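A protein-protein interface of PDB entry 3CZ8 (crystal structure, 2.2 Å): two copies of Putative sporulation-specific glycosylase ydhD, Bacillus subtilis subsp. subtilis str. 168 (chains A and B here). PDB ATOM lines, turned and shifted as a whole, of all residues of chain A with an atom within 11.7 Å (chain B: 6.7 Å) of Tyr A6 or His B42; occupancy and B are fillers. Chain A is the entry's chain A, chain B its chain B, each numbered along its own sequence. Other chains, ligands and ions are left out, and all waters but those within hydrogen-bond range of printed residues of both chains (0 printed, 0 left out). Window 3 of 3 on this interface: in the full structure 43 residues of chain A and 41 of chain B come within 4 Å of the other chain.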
ATOM      1  N   SER A   4       3.292  -6.209  11.288  1.00  0.00           N
ATOM      2  CA  SER A   4       3.947  -6.582   9.999  1.00  0.00           C
ATOM      3  C   SER A   4       2.952  -6.649   8.836  1.00  0.00           C
ATOM      4  O   SER A   4       1.765  -6.926   9.028  1.00  0.00           O
ATOM      5  CB  SER A   4       4.704  -7.908  10.137  1.00  0.00           C
ATOM      6  OG  SER A   4       3.834  -8.964  10.504  1.00  0.00           O
ATOM      7  N   ASN A   5       3.464  -6.393   7.633  1.00  0.00           N
ATOM      8  CA  ASN A   5       2.670  -6.311   6.411  1.00  0.00           C
ATOM      9  C   ASN A   5       3.602  -6.558   5.228  1.00  0.00           C
ATOM     10  O   ASN A   5       4.548  -5.793   5.019  1.00  0.00           O
ATOM     11  CB  ASN A   5       2.029  -4.912   6.303  1.00  0.00           C
ATOM     12  CG  ASN A   5       0.900  -4.833   5.270  1.00  0.00           C
ATOM     13  OD1 ASN A   5       0.765  -5.684   4.390  1.00  0.00           O
ATOM     14  ND2 ASN A   5       0.088  -3.784   5.377  1.00  0.00           N
ATOM     15  N   TYR A   6       3.362  -7.626   4.465  1.00  0.00           N
ATOM     16  CA  TYR A   6       4.105  -7.805   3.207  1.00  0.00           C
ATOM     17  C   TYR A   6       3.356  -7.371   1.953  1.00  0.00           C
ATOM     18  O   TYR A   6       3.616  -7.869   0.854  1.00  0.00           O
ATOM     19  CB  TYR A   6       4.753  -9.193   3.033  1.00  0.00           C
ATOM     20  CG  TYR A   6       4.401 -10.276   4.027  1.00  0.00           C
ATOM     21  CD1 TYR A   6       3.243 -11.038   3.881  1.00  0.00           C
ATOM     22  CD2 TYR A   6       5.263 -10.578   5.082  1.00  0.00           C
ATOM     23  CE1 TYR A   6       2.937 -12.055   4.781  1.00  0.00           C
ATOM     24  CE2 TYR A   6       4.966 -11.589   5.987  1.00  0.00           C
ATOM     25  CZ  TYR A   6       3.804 -12.323   5.831  1.00  0.00           C
ATOM     26  OH  TYR A   6       3.511 -13.323   6.728  1.00  0.00           O
ATOM     27  N   ILE A   7       2.417  -6.443   2.129  1.00  0.00           N
ATOM     28  CA  ILE A   7       1.994  -5.562   1.043  1.00  0.00           C
ATOM     29  C   ILE A   7       2.278  -4.120   1.483  1.00  0.00           C
ATOM     30  O   ILE A   7       1.452  -3.454   2.121  1.00  0.00           O
ATOM     31  CB  ILE A   7       0.530  -5.789   0.572  1.00  0.00           C
ATOM     32  CG1 ILE A   7       0.359  -7.214   0.038  1.00  0.00           C
ATOM     33  CG2 ILE A   7       0.155  -4.797  -0.537  1.00  0.00           C
ATOM     34  CD1 ILE A   7      -0.980  -7.492  -0.605  1.00  0.00           C
ATOM     35  N   ALA A   8       3.492  -3.678   1.172  1.00  0.00           N
ATOM     36  CA  ALA A   8       3.938  -2.321   1.442  1.00  0.00           C
ATOM     37  C   ALA A   8       4.600  -1.762   0.189  1.00  0.00           C
ATOM     38  O   ALA A   8       5.511  -2.378  -0.375  1.00  0.00           O
ATOM     39  CB  ALA A   8       4.904  -2.297   2.622  1.00  0.00           C
ATOM     40  N   GLY A   9       4.122  -0.603  -0.252  1.00  0.00           N
ATOM     41  CA  GLY A   9       4.652   0.041  -1.447  1.00  0.00           C
ATOM     42  C   GLY A   9       5.945   0.782  -1.182  1.00  0.00           C
ATOM     43  O   GLY A   9       6.011   1.634  -0.292  1.00  0.00           O
ATOM     44  N   THR A  10       6.979   0.445  -1.947  1.00  0.00           N
ATOM     45  CA  THR A  10       8.237   1.186  -1.924  1.00  0.00           C
ATOM     46  C   THR A  10       8.155   2.353  -2.909  1.00  0.00           C
ATOM     47  O   THR A  10       7.971   2.151  -4.115  1.00  0.00           O
ATOM     48  CB  THR A  10       9.443   0.282  -2.270  1.00  0.00           C
ATOM     49  OG1 THR A  10       9.481  -0.837  -1.374  1.00  0.00           O
ATOM     50  CG2 THR A  10      10.758   1.060  -2.168  1.00  0.00           C
ATOM     51  N   ASN A  54      15.531  -2.641   3.843  1.00  0.00           N
ATOM     52  CA  ASN A  54      15.691  -3.867   3.085  1.00  0.00           C
ATOM     53  C   ASN A  54      15.875  -3.495   1.622  1.00  0.00           C
ATOM     54  O   ASN A  54      14.981  -3.687   0.802  1.00  0.00           O
ATOM     55  CB  ASN A  54      14.487  -4.790   3.288  1.00  0.00           C
ATOM     56  CG  ASN A  54      14.758  -6.217   2.841  1.00  0.00           C
ATOM     57  OD1 ASN A  54      15.818  -6.781   3.120  1.00  0.00           O
ATOM     58  ND2 ASN A  54      13.791  -6.811   2.151  1.00  0.00           N
ATOM     59  N   THR A 309       6.701   0.196  -6.035  1.00  0.00           N
ATOM     60  CA  THR A 309       7.048  -1.204  -6.257  1.00  0.00           C
ATOM     61  C   THR A 309       6.727  -2.050  -5.026  1.00  0.00           C
ATOM     62  O   THR A 309       7.314  -1.865  -3.956  1.00  0.00           O
ATOM     63  CB  THR A 309       8.524  -1.363  -6.698  1.00  0.00           C
ATOM     64  OG1 THR A 309       8.717  -0.680  -7.945  1.00  0.00           O
ATOM     65  CG2 THR A 309       8.894  -2.832  -6.877  1.00  0.00           C
ATOM     66  N   LEU A 310       5.779  -2.967  -5.201  1.00  0.00           N
ATOM     67  CA  LEU A 310       5.325  -3.866  -4.142  1.00  0.00           C
ATOM     68  C   LEU A 310       6.265  -5.064  -4.018  1.00  0.00           C
ATOM     69  O   LEU A 310       6.578  -5.724  -5.012  1.00  0.00           O
ATOM     70  CB  LEU A 310       3.893  -4.335  -4.426  1.00  0.00           C
ATOM     71  CG  LEU A 310       2.675  -3.571  -3.883  1.00  0.00           C
ATOM     72  CD1 LEU A 310       2.645  -2.093  -4.261  1.00  0.00           C
ATOM     73  CD2 LEU A 310       1.402  -4.254  -4.359  1.00  0.00           C
ATOM     74  N   ALA A 311       6.715  -5.333  -2.796  1.00  0.00           N
ATOM     75  CA  ALA A 311       7.682  -6.401  -2.544  1.00  0.00           C
ATOM     76  C   ALA A 311       7.257  -7.295  -1.379  1.00  0.00           C
ATOM     77  O   ALA A 311       6.918  -6.811  -0.300  1.00  0.00           O
ATOM     78  CB  ALA A 311       9.072  -5.813  -2.296  1.00  0.00           C
ATOM     79  N   GLU B  40      -3.129  -5.932   4.310  1.00  0.00           N
ATOM     80  CA  GLU B  40      -3.906  -7.111   4.545  1.00  0.00           C
ATOM     81  C   GLU B  40      -3.694  -7.571   5.980  1.00  0.00           C
ATOM     82  O   GLU B  40      -2.817  -7.081   6.638  1.00  0.00           O
ATOM     83  CB  GLU B  40      -3.372  -8.192   3.639  1.00  0.00           C
ATOM     84  CG  GLU B  40      -1.910  -8.100   3.430  1.00  0.00           C
ATOM     85  CD  GLU B  40      -1.137  -8.949   4.346  1.00  0.00           C
ATOM     86  OE1 GLU B  40      -0.148  -8.485   4.879  1.00  0.00           O
ATOM     87  OE2 GLU B  40      -1.480 -10.094   4.529  1.00  0.00           O
ATOM     88  N   TYR B  41      -4.497  -8.522   6.444  1.00  0.00           N
ATOM     89  CA  TYR B  41      -4.121  -9.472   7.479  1.00  0.00           C
ATOM     90  C   TYR B  41      -3.917 -10.821   6.873  1.00  0.00           C
ATOM     91  O   TYR B  41      -4.593 -11.157   5.954  1.00  0.00           O
ATOM     92  CB  TYR B  41      -5.224  -9.587   8.516  1.00  0.00           C
ATOM     93  CG  TYR B  41      -5.420  -8.368   9.375  1.00  0.00           C
ATOM     94  CD1 TYR B  41      -6.224  -7.344   8.968  1.00  0.00           C
ATOM     95  CD2 TYR B  41      -4.809  -8.253  10.597  1.00  0.00           C
ATOM     96  CE1 TYR B  41      -6.398  -6.250   9.734  1.00  0.00           C
ATOM     97  CE2 TYR B  41      -4.989  -7.164  11.362  1.00  0.00           C
ATOM     98  CZ  TYR B  41      -5.778  -6.161  10.926  1.00  0.00           C
ATOM     99  OH  TYR B  41      -5.966  -5.048  11.672  1.00  0.00           O
ATOM    100  N   HIS B  42      -2.983 -11.605   7.383  1.00  0.00           N
ATOM    101  CA  HIS B  42      -2.755 -12.962   6.859  1.00  0.00           C
ATOM    102  C   HIS B  42      -2.933 -14.052   7.916  1.00  0.00           C
ATOM    103  O   HIS B  42      -2.961 -13.771   9.118  1.00  0.00           O
ATOM    104  CB  HIS B  42      -1.394 -13.092   6.169  1.00  0.00           C
ATOM    105  CG  HIS B  42      -0.263 -12.493   6.945  1.00  0.00           C
ATOM    106  ND1 HIS B  42       0.162 -11.196   6.757  1.00  0.00           N
ATOM    107  CD2 HIS B  42       0.529 -13.013   7.912  1.00  0.00           C
ATOM    108  CE1 HIS B  42       1.170 -10.943   7.572  1.00  0.00           C
ATOM    109  NE2 HIS B  42       1.411 -12.028   8.285  1.00  0.00           N
ATOM    110  N   ILE B  43      -3.045 -15.298   7.453  1.00  0.00           N
ATOM    111  CA  ILE B  43      -3.498 -16.403   8.302  1.00  0.00           C
ATOM    112  C   ILE B  43      -2.442 -17.473   8.601  1.00  0.00           C
ATOM    113  O   ILE B  43      -1.603 -17.807   7.757  1.00  0.00           O
ATOM    114  CB  ILE B  43      -4.800 -17.066   7.752  1.00  0.00           C
ATOM    115  CG1 ILE B  43      -4.580 -17.684   6.365  1.00  0.00           C
ATOM    116  CG2 ILE B  43      -5.923 -16.046   7.697  1.00  0.00           C
ATOM    117  CD1 ILE B  43      -5.537 -18.828   6.020  1.00  0.00           C
ATOM    118  N   ALA B  44      -2.496 -17.990   9.824  1.00  0.00           N
ATOM    119  CA  ALA B  44      -1.674 -19.115  10.247  1.00  0.00           C
ATOM    120  C   ALA B  44      -2.474 -20.396   9.981  1.00  0.00           C
ATOM    121  O   ALA B  44      -3.704 -20.326   9.895  1.00  0.00           O
ATOM    122  CB  ALA B  44      -1.323 -18.963  11.724  1.00  0.00           C
ATOM    123  N   ASP B  48      -5.342 -18.797  12.984  1.00  0.00           N
ATOM    124  CA  ASP B  48      -5.081 -17.557  13.705  1.00  0.00           C
ATOM    125  C   ASP B  48      -4.762 -16.423  12.741  1.00  0.00           C
ATOM    126  O   ASP B  48      -4.275 -16.657  11.633  1.00  0.00           O
ATOM    127  CB  ASP B  48      -3.921 -17.750  14.693  1.00  0.00           C
ATOM    128  CG  ASP B  48      -4.392 -18.078  16.103  1.00  0.00           C
ATOM    129  OD1 ASP B  48      -5.334 -18.887  16.261  1.00  0.00           O
ATOM    130  OD2 ASP B  48      -3.809 -17.525  17.060  1.00  0.00           O
ATOM    131  N   ILE B  49      -5.043 -15.194  13.161  1.00  0.00           N
ATOM    132  CA  ILE B  49      -4.611 -14.028  12.404  1.00  0.00           C
ATOM    133  C   ILE B  49      -3.227 -13.628  12.907  1.00  0.00           C
ATOM    134  O   ILE B  49      -3.058 -13.242  14.068  1.00  0.00           O
ATOM    135  CB  ILE B  49      -5.633 -12.868  12.470  1.00  0.00           C
ATOM    136  CG1 ILE B  49      -6.926 -13.282  11.757  1.00  0.00           C
ATOM    137  CG2 ILE B  49      -5.050 -11.600  11.840  1.00  0.00           C
ATOM    138  CD1 ILE B  49      -8.049 -12.282  11.855  1.00  0.00           C
ATOM    139  N   ALA B  50      -2.248 -13.740  12.014  1.00  0.00           N
ATOM    140  CA  ALA B  50      -0.830 -13.660  12.362  1.00  0.00           C
ATOM    141  C   ALA B  50      -0.301 -12.260  12.655  1.00  0.00           C
ATOM    142  O   ALA B  50       0.633 -12.108  13.443  1.00  0.00           O
ATOM    143  CB  ALA B  50       0.008 -14.323  11.280  1.00  0.00           C
ATOM    144  N   ASN B  51      -0.886 -11.241  12.030  1.00  0.00           N
ATOM    145  CA  ASN B  51      -0.330  -9.888  12.115  1.00  0.00           C
ATOM    146  C   ASN B  51      -1.269  -8.819  12.670  1.00  0.00           C
ATOM    147  O   ASN B  51      -2.477  -9.028  12.779  1.00  0.00           O
ATOM    148  CB  ASN B  51       0.219  -9.448  10.752  1.00  0.00           C
ATOM    149  CG  ASN B  51      -0.857  -9.370   9.687  1.00  0.00           C
ATOM    150  OD1 ASN B  51      -1.484 -10.375   9.345  1.00  0.00           O
ATOM    151  ND2 ASN B  51      -1.066  -8.175   9.144  1.00  0.00           N
ATOM    152  N   GLN B  52      -0.686  -7.677  13.024  1.00  0.00           N
ATOM    153  CA  GLN B  52      -1.440  -6.506  13.454  1.00  0.00           C
ATOM    154  C   GLN B  52      -1.171  -5.359  12.498  1.00  0.00           C
ATOM    155  O   GLN B  52      -0.109  -5.298  11.872  1.00  0.00           O
ATOM    156  CB  GLN B  52      -1.046  -6.096  14.875  1.00  0.00           C
ATOM    157  CG  GLN B  52      -1.655  -6.967  15.970  1.00  0.00           C
ATOM    158  CD  GLN B  52      -1.265  -6.520  17.371  1.00  0.00           C
ATOM    159  OE1 GLN B  52      -2.128  -6.221  18.200  1.00  0.00           O
ATOM    160  NE2 GLN B  52       0.037  -6.472  17.641  1.00  0.00           N
ATOM    161  N   THR B  72      -9.092  -6.866   4.714  1.00  0.00           N
ATOM    162  CA  THR B  72      -8.692  -7.870   3.735  1.00  0.00           C
ATOM    163  C   THR B  72      -7.962  -8.990   4.457  1.00  0.00           C
ATOM    164  O   THR B  72      -7.029  -8.743   5.225  1.00  0.00           O
ATOM    165  CB  THR B  72      -7.820  -7.267   2.603  1.00  0.00           C
ATOM    166  OG1 THR B  72      -8.469  -6.102   2.075  1.00  0.00           O
ATOM    167  CG2 THR B  72      -7.608  -8.270   1.472  1.00  0.00           C
ATOM    168  N   ILE B  73      -8.412 -10.217   4.220  1.00  0.00           N
ATOM    169  CA  ILE B  73      -7.849 -11.400   4.856  1.00  0.00           C
ATOM    170  C   ILE B  73      -7.224 -12.262   3.763  1.00  0.00           C
ATOM    171  O   ILE B  73      -7.919 -12.693   2.842  1.00  0.00           O
ATOM    172  CB  ILE B  73      -8.942 -12.215   5.640  1.00  0.00           C
ATOM    173  CG1 ILE B  73      -9.830 -11.302   6.508  1.00  0.00           C
ATOM    174  CG2 ILE B  73      -8.316 -13.339   6.464  1.00  0.00           C
ATOM    175  CD1 ILE B  73      -9.099 -10.472   7.584  1.00  0.00           C
ATOM    176  N   THR B  74      -5.914 -12.497   3.865  1.00  0.00           N
ATOM    177  CA  THR B  74      -5.159 -13.213   2.827  1.00  0.00           C
ATOM    178  C   THR B  74      -4.476 -14.486   3.328  1.00  0.00           C
ATOM    179  O   THR B  74      -4.340 -14.696   4.533  1.00  0.00           O
ATOM    180  CB  THR B  74      -4.078 -12.308   2.153  1.00  0.00           C
ATOM    181  OG1 THR B  74      -3.111 -11.881   3.124  1.00  0.00           O
ATOM    182  CG2 THR B  74      -4.709 -11.090   1.490  1.00  0.00           C
ATOM    183  N   ASN B  75      -4.057 -15.332   2.389  1.00  0.00           N
ATOM    184  CA  ASN B  75      -3.185 -16.474   2.683  1.00  0.00           C
ATOM    185  C   ASN B  75      -1.746 -16.173   2.244  1.00  0.00           C
ATOM    186  O   ASN B  75      -1.086 -16.976   1.581  1.00  0.00           O
ATOM    187  CB  ASN B  75      -3.711 -17.756   2.024  1.00  0.00           C
ATOM    188  CG  ASN B  75      -3.922 -17.605   0.524  1.00  0.00           C
ATOM    189  OD1 ASN B  75      -4.370 -16.564   0.052  1.00  0.00           O
ATOM    190  ND2 ASN B  75      -3.595 -18.651  -0.229  1.00  0.00           N
ATOM    191  N   LEU B  76      -1.269 -15.002   2.638  1.00  0.00           N
ATOM    192  CA  LEU B  76       0.006 -14.482   2.177  1.00  0.00           C
ATOM    193  C   LEU B  76       1.135 -14.884   3.121  1.00  0.00           C
ATOM    194  O   LEU B  76       0.941 -14.952   4.339  1.00  0.00           O
ATOM    195  CB  LEU B  76      -0.091 -12.962   2.076  1.00  0.00           C
ATOM    196  CG  LEU B  76       0.512 -12.176   0.911  1.00  0.00           C
ATOM    197  CD1 LEU B  76       0.507 -12.932  -0.400  1.00  0.00           C
ATOM    198  CD2 LEU B  76      -0.270 -10.895   0.771  1.00  0.00           C
ATOM    199  N   THR B  77       2.306 -15.165   2.548  1.00  0.00           N
ATOM    200  CA  THR B  77       3.504 -15.516   3.317  1.00  0.00           C
ATOM    201  C   THR B  77       4.707 -14.674   2.900  1.00  0.00           C
ATOM    202  O   THR B  77       4.555 -13.580   2.347  1.00  0.00           O
ATOM    203  CB  THR B  77       3.884 -17.010   3.163  1.00  0.00           C
ATOM    204  OG1 THR B  77       3.981 -17.347   1.774  1.00  0.00           O
ATOM    205  CG2 THR B  77       2.870 -17.904   3.837  1.00  0.00           C
ATOM    206  N   SER B  78       5.899 -15.205   3.173  1.00  0.00           N
ATOM    207  CA  SER B  78       7.167 -14.569   2.818  1.00  0.00           C
ATOM    208  C   SER B  78       7.385 -14.532   1.304  1.00  0.00           C
ATOM    209  O   SER B  78       7.885 -13.540   0.771  1.00  0.00           O
ATOM    210  CB  SER B  78       8.332 -15.299   3.494  1.00  0.00           C
ATOM    211  OG  SER B  78       8.100 -15.469   4.882  1.00  0.00           O
ATOM    212  N   GLY B  80       4.900 -14.998  -1.268  1.00  0.00           N
ATOM    213  CA  GLY B  80       3.624 -14.954  -1.985  1.00  0.00           C
ATOM    214  C   GLY B  80       2.496 -15.735  -1.332  1.00  0.00           C
ATOM    215  O   GLY B  80       2.536 -16.030  -0.133  1.00  0.00           O
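O of Ser A4 sits at hydrogen-bond distance from ND2 of Asn B51.
The side-chain carboxylate of Glu B40 lies close to the side-chain amide oxygen of Asn A5 (3.0 Å).
NE2 of His B42 sits at hydrogen-bond distance from OH of Tyr A6.
The backbone NH of Ile A7 is in hydrogen-bond range of the side-chain amide oxygen of Asn A5, at 2.9 Å.
OE2 of Glu B40 lies within hydrogen-bond range of ND1 of His B42 (3.0 Å).
OE2 of Glu B40 lies within hydrogen-bond range of OG1 of Thr B74 (2.8 Å).
N of Ala B50 lies within hydrogen-bond range of O of His B42 (3.0 Å).
N of His B42 lies within hydrogen-bond range of OD1 of Asn B51 (2.8 Å).
The side-chain hydroxyl of Thr B77 sits at hydrogen-bond distance from the backbone carbonyl oxygen of Gly B80 (2.7 Å).
N of Ser A4 touches O of Gln B52, 3.6 Å away.
OE1 of Glu B40 touches N of Tyr A6 (3.6 Å).
Leu B76 touches Tyr A6 (O to CE1, 3.5 Å).
Tyr A6 touches Thr B77.
CD2 of Leu B76 touches CD1 of Ile A7 (3.7 Å).
Printed residues of chain B within 4 Å of Ser A4: Asn B51 (3.1 Å) and Gln B52 (3.6 Å).
Of the printed residues of chain B, Asn A5 touches Glu B40 (3.0 Å).
Printed residues of chain B within 4 Å of Tyr A6: Glu B40, His B42, Leu B76 and Thr B77.
His B42 touches just one residue of chain A: Tyr A6 (2.9 Å).
Ile B43 touches none of the printed residues of chain A.
No residue of chain A comes within 4 Å of Ile B49.
No residue of chain A comes within 4 Å of Ala B50.
Asn B51 touches just one residue of chain A: Ser A4.
Ile B73 touches none of the printed residues of chain A.
Thr B74 touches none of the printed residues of chain A.
Leu B76 touches just these residues of chain A: Tyr A6 and Ile A7.
Of chain A, only Tyr A6 (3.2 Å) comes within 4 Å of Thr B77.
No residue of chain A comes within 4 Å of Ser B78.
The nearest printed residue of chain B that does not touch Ser A4 is His B42 (4.3 Å).
Of the 11 printed residues of chain A, 4 touch a printed residue of chain B.
Of the 18 printed residues of chain B, 6 touch a printed residue of chain A.
Hydrophobic or aromatic side chains of chain B that line the printed part of chain A: His B42 and Leu B76.
No position is printed for both chains.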
